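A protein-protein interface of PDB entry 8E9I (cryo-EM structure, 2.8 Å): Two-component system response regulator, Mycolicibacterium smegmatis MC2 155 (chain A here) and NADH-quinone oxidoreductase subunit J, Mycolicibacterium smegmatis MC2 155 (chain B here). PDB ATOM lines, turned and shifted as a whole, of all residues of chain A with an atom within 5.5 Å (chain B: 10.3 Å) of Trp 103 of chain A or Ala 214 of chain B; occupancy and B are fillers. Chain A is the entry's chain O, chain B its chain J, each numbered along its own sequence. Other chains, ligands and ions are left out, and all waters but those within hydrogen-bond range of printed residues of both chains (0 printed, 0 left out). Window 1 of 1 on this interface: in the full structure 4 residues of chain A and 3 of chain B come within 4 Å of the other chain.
Printed residues of chain B that touch a printed residue of chain A: Tyr 213, Ala 214 and Arg 215.
Hydrophobic or aromatic side chains of chain A that line the printed part of chain B: Trp 99.
Among the printed residues, 6 pairs touch across the chains.
Among the printed residues, no Asp or Glu carboxylate lies within 4 Å of a Lys or Arg side-chain nitrogen of the other chain.
The backbone carbonyl oxygen of Lys 102 of chain A sits at hydrogen-bond distance from the guanidinium group of Arg 215 of chain B (2.5 Å).
The backbone carbonyl oxygen (O) of Arg 215 of chain B lies within hydrogen-bond range of the guanidinium group (NH2) of Arg 105 of chain A, at 3.0 Å.
N of Ala 214 of chain B sits close to NE1 of Trp 99 of chain A (3.5 Å).
No residue of chain B comes within 4 Å of Gly 73 of chain A.
Trp 99 of chain A touches just these residues of chain B: Tyr 213 (3.8 Å) and Ala 214 (3.5 Å).
No residue of chain B comes within 4 Å of Leu 100 of chain A.
Ala 101 of chain A touches none of the printed residues of chain B.
Of chain B, only Ala 214 (3.6 Å) and Arg 215 (2.5 Å) come within 4 Å of Lys 102 of chain A.
Of chain B, only Ala 214 comes within 4 Å of Trp 103 of chain A.
No residue of chain B comes within 4 Å of Ser 104 of chain A.
Printed residues of chain B within 4 Å of Arg 105 of chain A: Arg 215.
Of the printed residues of chain A, Tyr 213 of chain B touches Trp 99 (3.8 Å).
Printed residues of chain A within 4 Å of Arg 215 of chain B: Lys 102 and Arg 105.
The nearest residue of chain B that does not touch Trp 103 of chain A is Arg 215 of chain B (4.1 Å).
The nearest printed residue of chain A that does not touch Ala 214 of chain B is Arg 105 of chain A (5.5 Å).
The nearest printed residue of chain A that does not touch Arg 215 of chain B is Trp 103 of chain A (4.1 Å).
CZ2 of Trp 99 of chain A touches C of Tyr 213 of chain B (3.8 Å).
Ala 214 of chain B touches Lys 102 of chain A.
CB of Ala 214 of chain B touches N of Trp 103 of chain A, at 3.6 Å.
The backbone carbonyl oxygen (O) of Trp 103 of chain A lies within hydrogen-bond range of the guanidinium group (NH1) of Arg 105 of chain A (2.7 Å).
O of Pro 222 of chain B is in hydrogen-bond range of OH of Tyr 213 of chain B, at 3.1 Å.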
ATOM      1  N   MET A  72      14.568   7.522 -30.240  1.00  0.00           N
ATOM      2  CA  MET A  72      13.721   6.486 -29.658  1.00  0.00           C
ATOM      3  C   MET A  72      14.066   6.256 -28.195  1.00  0.00           C
ATOM      4  O   MET A  72      13.171   6.128 -27.350  1.00  0.00           O
ATOM      5  CB  MET A  72      13.862   5.194 -30.455  1.00  0.00           C
ATOM      6  CG  MET A  72      13.321   5.300 -31.860  1.00  0.00           C
ATOM      7  SD  MET A  72      13.444   3.752 -32.753  1.00  0.00           S
ATOM      8  CE  MET A  72      15.202   3.721 -33.075  1.00  0.00           C
ATOM      9  N   GLY A  73      15.357   6.197 -27.875  1.00  0.00           N
ATOM     10  CA  GLY A  73      15.747   6.103 -26.481  1.00  0.00           C
ATOM     11  C   GLY A  73      15.281   7.303 -25.685  1.00  0.00           C
ATOM     12  O   GLY A  73      14.776   7.164 -24.567  1.00  0.00           O
ATOM     13  N   LYS A  76      11.457   6.897 -25.075  1.00  0.00           N
ATOM     14  CA  LYS A  76      11.140   6.012 -23.964  1.00  0.00           C
ATOM     15  C   LYS A  76      11.479   6.676 -22.638  1.00  0.00           C
ATOM     16  O   LYS A  76      10.690   6.627 -21.687  1.00  0.00           O
ATOM     17  CB  LYS A  76      11.890   4.691 -24.113  1.00  0.00           C
ATOM     18  CG  LYS A  76      11.504   3.632 -23.095  1.00  0.00           C
ATOM     19  CD  LYS A  76      10.033   3.263 -23.202  1.00  0.00           C
ATOM     20  CE  LYS A  76       9.695   2.072 -22.332  1.00  0.00           C
ATOM     21  NZ  LYS A  76       9.664   2.441 -20.893  1.00  0.00           N
ATOM     22  N   ALA A  98      10.622   0.384 -37.399  1.00  0.00           N
ATOM     23  CA  ALA A  98       9.248   0.597 -36.969  1.00  0.00           C
ATOM     24  C   ALA A  98       8.981  -0.117 -35.658  1.00  0.00           C
ATOM     25  O   ALA A  98       8.363   0.451 -34.752  1.00  0.00           O
ATOM     26  CB  ALA A  98       8.267   0.106 -38.032  1.00  0.00           C
ATOM     27  N   TRP A  99       9.450  -1.359 -35.540  1.00  0.00           N
ATOM     28  CA  TRP A  99       9.210  -2.103 -34.313  1.00  0.00           C
ATOM     29  C   TRP A  99       9.735  -1.336 -33.110  1.00  0.00           C
ATOM     30  O   TRP A  99       9.012  -1.141 -32.129  1.00  0.00           O
ATOM     31  CB  TRP A  99       9.852  -3.484 -34.408  1.00  0.00           C
ATOM     32  CG  TRP A  99       9.456  -4.408 -33.308  1.00  0.00           C
ATOM     33  CD1 TRP A  99       8.314  -5.139 -33.237  1.00  0.00           C
ATOM     34  CD2 TRP A  99      10.201  -4.713 -32.131  1.00  0.00           C
ATOM     35  NE1 TRP A  99       8.295  -5.878 -32.086  1.00  0.00           N
ATOM     36  CE2 TRP A  99       9.446  -5.634 -31.388  1.00  0.00           C
ATOM     37  CE3 TRP A  99      11.435  -4.296 -31.631  1.00  0.00           C
ATOM     38  CZ2 TRP A  99       9.881  -6.144 -30.174  1.00  0.00           C
ATOM     39  CZ3 TRP A  99      11.865  -4.802 -30.428  1.00  0.00           C
ATOM     40  CH2 TRP A  99      11.091  -5.715 -29.710  1.00  0.00           C
ATOM     41  N   LEU A 100      10.972  -0.844 -33.184  1.00  0.00           N
ATOM     42  CA  LEU A 100      11.490  -0.039 -32.087  1.00  0.00           C
ATOM     43  C   LEU A 100      10.658   1.213 -31.875  1.00  0.00           C
ATOM     44  O   LEU A 100      10.418   1.606 -30.728  1.00  0.00           O
ATOM     45  CB  LEU A 100      12.949   0.327 -32.336  1.00  0.00           C
ATOM     46  CG  LEU A 100      13.931  -0.810 -32.079  1.00  0.00           C
ATOM     47  CD1 LEU A 100      15.344  -0.363 -32.371  1.00  0.00           C
ATOM     48  CD2 LEU A 100      13.820  -1.300 -30.644  1.00  0.00           C
ATOM     49  N   ALA A 101      10.195   1.841 -32.952  1.00  0.00           N
ATOM     50  CA  ALA A 101       9.302   2.980 -32.792  1.00  0.00           C
ATOM     51  C   ALA A 101       8.035   2.572 -32.052  1.00  0.00           C
ATOM     52  O   ALA A 101       7.505   3.341 -31.243  1.00  0.00           O
ATOM     53  CB  ALA A 101       8.965   3.578 -34.153  1.00  0.00           C
ATOM     54  N   LYS A 102       7.535   1.362 -32.310  1.00  0.00           N
ATOM     55  CA  LYS A 102       6.421   0.862 -31.516  1.00  0.00           C
ATOM     56  C   LYS A 102       6.821   0.733 -30.053  1.00  0.00           C
ATOM     57  O   LYS A 102       6.047   1.086 -29.156  1.00  0.00           O
ATOM     58  CB  LYS A 102       5.938  -0.478 -32.066  1.00  0.00           C
ATOM     59  N   TRP A 103       8.035   0.243 -29.793  1.00  0.00           N
ATOM     60  CA  TRP A 103       8.488   0.077 -28.416  1.00  0.00           C
ATOM     61  C   TRP A 103       8.720   1.421 -27.746  1.00  0.00           C
ATOM     62  O   TRP A 103       8.496   1.568 -26.540  1.00  0.00           O
ATOM     63  CB  TRP A 103       9.763  -0.762 -28.379  1.00  0.00           C
ATOM     64  CG  TRP A 103      10.564  -0.586 -27.128  1.00  0.00           C
ATOM     65  CD1 TRP A 103      10.348  -1.189 -25.928  1.00  0.00           C
ATOM     66  CD2 TRP A 103      11.716   0.243 -26.958  1.00  0.00           C
ATOM     67  NE1 TRP A 103      11.290  -0.786 -25.018  1.00  0.00           N
ATOM     68  CE2 TRP A 103      12.143   0.093 -25.628  1.00  0.00           C
ATOM     69  CE3 TRP A 103      12.427   1.100 -27.800  1.00  0.00           C
ATOM     70  CZ2 TRP A 103      13.244   0.768 -25.121  1.00  0.00           C
ATOM     71  CZ3 TRP A 103      13.520   1.767 -27.292  1.00  0.00           C
ATOM     72  CH2 TRP A 103      13.919   1.598 -25.968  1.00  0.00           C
ATOM     73  N   SER A 104       9.166   2.417 -28.507  1.00  0.00           N
ATOM     74  CA  SER A 104       9.364   3.743 -27.944  1.00  0.00           C
ATOM     75  C   SER A 104       8.064   4.383 -27.490  1.00  0.00           C
ATOM     76  O   SER A 104       8.107   5.402 -26.797  1.00  0.00           O
ATOM     77  CB  SER A 104      10.042   4.649 -28.968  1.00  0.00           C
ATOM     78  OG  SER A 104       9.096   5.161 -29.885  1.00  0.00           O
ATOM     79  N   ARG A 105       6.919   3.828 -27.877  1.00  0.00           N
ATOM     80  CA  ARG A 105       5.610   4.303 -27.444  1.00  0.00           C
ATOM     81  C   ARG A 105       5.287   5.683 -27.990  1.00  0.00           C
ATOM     82  O   ARG A 105       4.316   6.310 -27.561  1.00  0.00           O
ATOM     83  CB  ARG A 105       5.504   4.300 -25.918  1.00  0.00           C
ATOM     84  CG  ARG A 105       5.391   2.912 -25.347  1.00  0.00           C
ATOM     85  CD  ARG A 105       6.067   2.806 -24.006  1.00  0.00           C
ATOM     86  NE  ARG A 105       5.766   1.533 -23.363  1.00  0.00           N
ATOM     87  CZ  ARG A 105       6.487   0.428 -23.498  1.00  0.00           C
ATOM     88  NH1 ARG A 105       7.548   0.384 -24.288  1.00  0.00           N
ATOM     89  NH2 ARG A 105       6.131  -0.662 -22.827  1.00  0.00           N
ATOM     90  N   GLY B 211       5.435 -14.741 -25.507  1.00  0.00           N
ATOM     91  CA  GLY B 211       5.687 -13.906 -26.657  1.00  0.00           C
ATOM     92  C   GLY B 211       6.415 -12.629 -26.291  1.00  0.00           C
ATOM     93  O   GLY B 211       6.337 -12.134 -25.168  1.00  0.00           O
ATOM     94  N   VAL B 212       7.145 -12.097 -27.266  1.00  0.00           N
ATOM     95  CA  VAL B 212       7.837 -10.821 -27.138  1.00  0.00           C
ATOM     96  C   VAL B 212       7.208  -9.859 -28.127  1.00  0.00           C
ATOM     97  O   VAL B 212       7.196 -10.120 -29.335  1.00  0.00           O
ATOM     98  CB  VAL B 212       9.343 -10.956 -27.391  1.00  0.00           C
ATOM     99  CG1 VAL B 212      10.013  -9.600 -27.296  1.00  0.00           C
ATOM    100  CG2 VAL B 212       9.951 -11.927 -26.406  1.00  0.00           C
ATOM    101  N   TYR B 213       6.679  -8.756 -27.615  1.00  0.00           N
ATOM    102  CA  TYR B 213       6.067  -7.724 -28.429  1.00  0.00           C
ATOM    103  C   TYR B 213       6.745  -6.404 -28.122  1.00  0.00           C
ATOM    104  O   TYR B 213       7.351  -6.235 -27.063  1.00  0.00           O
ATOM    105  CB  TYR B 213       4.574  -7.591 -28.146  1.00  0.00           C
ATOM    106  CG  TYR B 213       3.765  -8.817 -28.458  1.00  0.00           C
ATOM    107  CD1 TYR B 213       3.886  -9.962 -27.694  1.00  0.00           C
ATOM    108  CD2 TYR B 213       2.865  -8.822 -29.506  1.00  0.00           C
ATOM    109  CE1 TYR B 213       3.149 -11.080 -27.974  1.00  0.00           C
ATOM    110  CE2 TYR B 213       2.122  -9.938 -29.794  1.00  0.00           C
ATOM    111  CZ  TYR B 213       2.265 -11.065 -29.023  1.00  0.00           C
ATOM    112  OH  TYR B 213       1.521 -12.187 -29.303  1.00  0.00           O
ATOM    113  N   ALA B 214       6.652  -5.472 -29.059  1.00  0.00           N
ATOM    114  CA  ALA B 214       6.961  -4.097 -28.718  1.00  0.00           C
ATOM    115  C   ALA B 214       5.996  -3.651 -27.634  1.00  0.00           C
ATOM    116  O   ALA B 214       4.785  -3.859 -27.745  1.00  0.00           O
ATOM    117  CB  ALA B 214       6.846  -3.201 -29.945  1.00  0.00           C
ATOM    118  N   ARG B 215       6.531  -3.053 -26.579  1.00  0.00           N
ATOM    119  CA  ARG B 215       5.799  -2.547 -25.428  1.00  0.00           C
ATOM    120  C   ARG B 215       5.391  -3.651 -24.454  1.00  0.00           C
ATOM    121  O   ARG B 215       4.844  -3.335 -23.398  1.00  0.00           O
ATOM    122  CB  ARG B 215       4.534  -1.761 -25.823  1.00  0.00           C
ATOM    123  CG  ARG B 215       4.751  -0.731 -26.916  1.00  0.00           C
ATOM    124  CD  ARG B 215       3.448  -0.088 -27.339  1.00  0.00           C
ATOM    125  NE  ARG B 215       3.643   0.852 -28.434  1.00  0.00           N
ATOM    126  CZ  ARG B 215       2.663   1.373 -29.159  1.00  0.00           C
ATOM    127  NH1 ARG B 215       1.398   1.036 -28.959  1.00  0.00           N
ATOM    128  NH2 ARG B 215       2.957   2.257 -30.108  1.00  0.00           N
ATOM    129  N   HIS B 216       5.627  -4.925 -24.756  1.00  0.00           N
ATOM    130  CA  HIS B 216       5.239  -5.999 -23.845  1.00  0.00           C
ATOM    131  C   HIS B 216       6.138  -7.200 -24.067  1.00  0.00           C
ATOM    132  O   HIS B 216       6.052  -7.853 -25.109  1.00  0.00           O
ATOM    133  CB  HIS B 216       3.778  -6.400 -24.049  1.00  0.00           C
ATOM    134  CG  HIS B 216       2.814  -5.271 -23.893  1.00  0.00           C
ATOM    135  ND1 HIS B 216       2.531  -4.700 -22.672  1.00  0.00           N
ATOM    136  CD2 HIS B 216       2.065  -4.607 -24.804  1.00  0.00           C
ATOM    137  CE1 HIS B 216       1.650  -3.729 -22.837  1.00  0.00           C
ATOM    138  NE2 HIS B 216       1.350  -3.653 -24.121  1.00  0.00           N
ATOM    139  N   ASN B 217       6.983  -7.501 -23.084  1.00  0.00           N
ATOM    140  CA  ASN B 217       7.817  -8.693 -23.147  1.00  0.00           C
ATOM    141  C   ASN B 217       7.718  -9.534 -21.881  1.00  0.00           C
ATOM    142  O   ASN B 217       8.402 -10.559 -21.784  1.00  0.00           O
ATOM    143  CB  ASN B 217       9.274  -8.309 -23.398  1.00  0.00           C
ATOM    144  CG  ASN B 217       9.818  -7.379 -22.344  1.00  0.00           C
ATOM    145  OD1 ASN B 217       9.363  -7.384 -21.203  1.00  0.00           O
ATOM    146  ND2 ASN B 217      10.799  -6.573 -22.716  1.00  0.00           N
ATOM    147  N   SER B 218       6.893  -9.138 -20.918  1.00  0.00           N
ATOM    148  CA  SER B 218       6.797  -9.854 -19.659  1.00  0.00           C
ATOM    149  C   SER B 218       6.379 -11.303 -19.889  1.00  0.00           C
ATOM    150  O   SER B 218       5.872 -11.675 -20.949  1.00  0.00           O
ATOM    151  CB  SER B 218       5.797  -9.163 -18.733  1.00  0.00           C
ATOM    152  OG  SER B 218       4.588  -8.881 -19.408  1.00  0.00           O
ATOM    153  N   VAL B 221       2.830 -12.497 -21.220  1.00  0.00           N
ATOM    154  CA  VAL B 221       2.424 -12.199 -22.590  1.00  0.00           C
ATOM    155  C   VAL B 221       2.345 -13.490 -23.399  1.00  0.00           C
ATOM    156  O   VAL B 221       3.366 -14.170 -23.564  1.00  0.00           O
ATOM    157  CB  VAL B 221       3.405 -11.210 -23.235  1.00  0.00           C
ATOM    158  CG1 VAL B 221       2.971 -10.873 -24.643  1.00  0.00           C
ATOM    159  CG2 VAL B 221       3.532  -9.959 -22.384  1.00  0.00           C
ATOM    160  N   PRO B 222       1.183 -13.866 -23.932  1.00  0.00           N
ATOM    161  CA  PRO B 222       1.114 -15.093 -24.731  1.00  0.00           C
ATOM    162  C   PRO B 222       1.664 -14.883 -26.132  1.00  0.00           C
ATOM    163  O   PRO B 222       1.555 -13.799 -26.708  1.00  0.00           O
ATOM    164  CB  PRO B 222      -0.383 -15.408 -24.758  1.00  0.00           C
ATOM    165  CG  PRO B 222      -1.028 -14.089 -24.660  1.00  0.00           C
ATOM    166  CD  PRO B 222      -0.144 -13.246 -23.779  1.00  0.00           C
ATOM    167  N   ARG B 224       2.150 -15.549 -30.297  1.00  0.00           N
ATOM    168  CA  ARG B 224       1.213 -15.484 -31.410  1.00  0.00           C
ATOM    169  C   ARG B 224       1.461 -16.626 -32.387  1.00  0.00           C
ATOM    170  O   ARG B 224       2.571 -16.780 -32.903  1.00  0.00           O
ATOM    171  CB  ARG B 224       1.338 -14.145 -32.133  1.00  0.00           C
ATOM    172  CG  ARG B 224       0.383 -13.983 -33.298  1.00  0.00           C
ATOM    173  CD  ARG B 224       0.565 -12.640 -33.972  1.00  0.00           C
ATOM    174  NE  ARG B 224       0.120 -11.545 -33.121  1.00  0.00           N
ATOM    175  CZ  ARG B 224       0.538 -10.291 -33.232  1.00  0.00           C
ATOM    176  NH1 ARG B 224       1.403  -9.929 -34.163  1.00  0.00           N
ATOM    177  NH2 ARG B 224       0.074  -9.377 -32.384  1.00  0.00           N
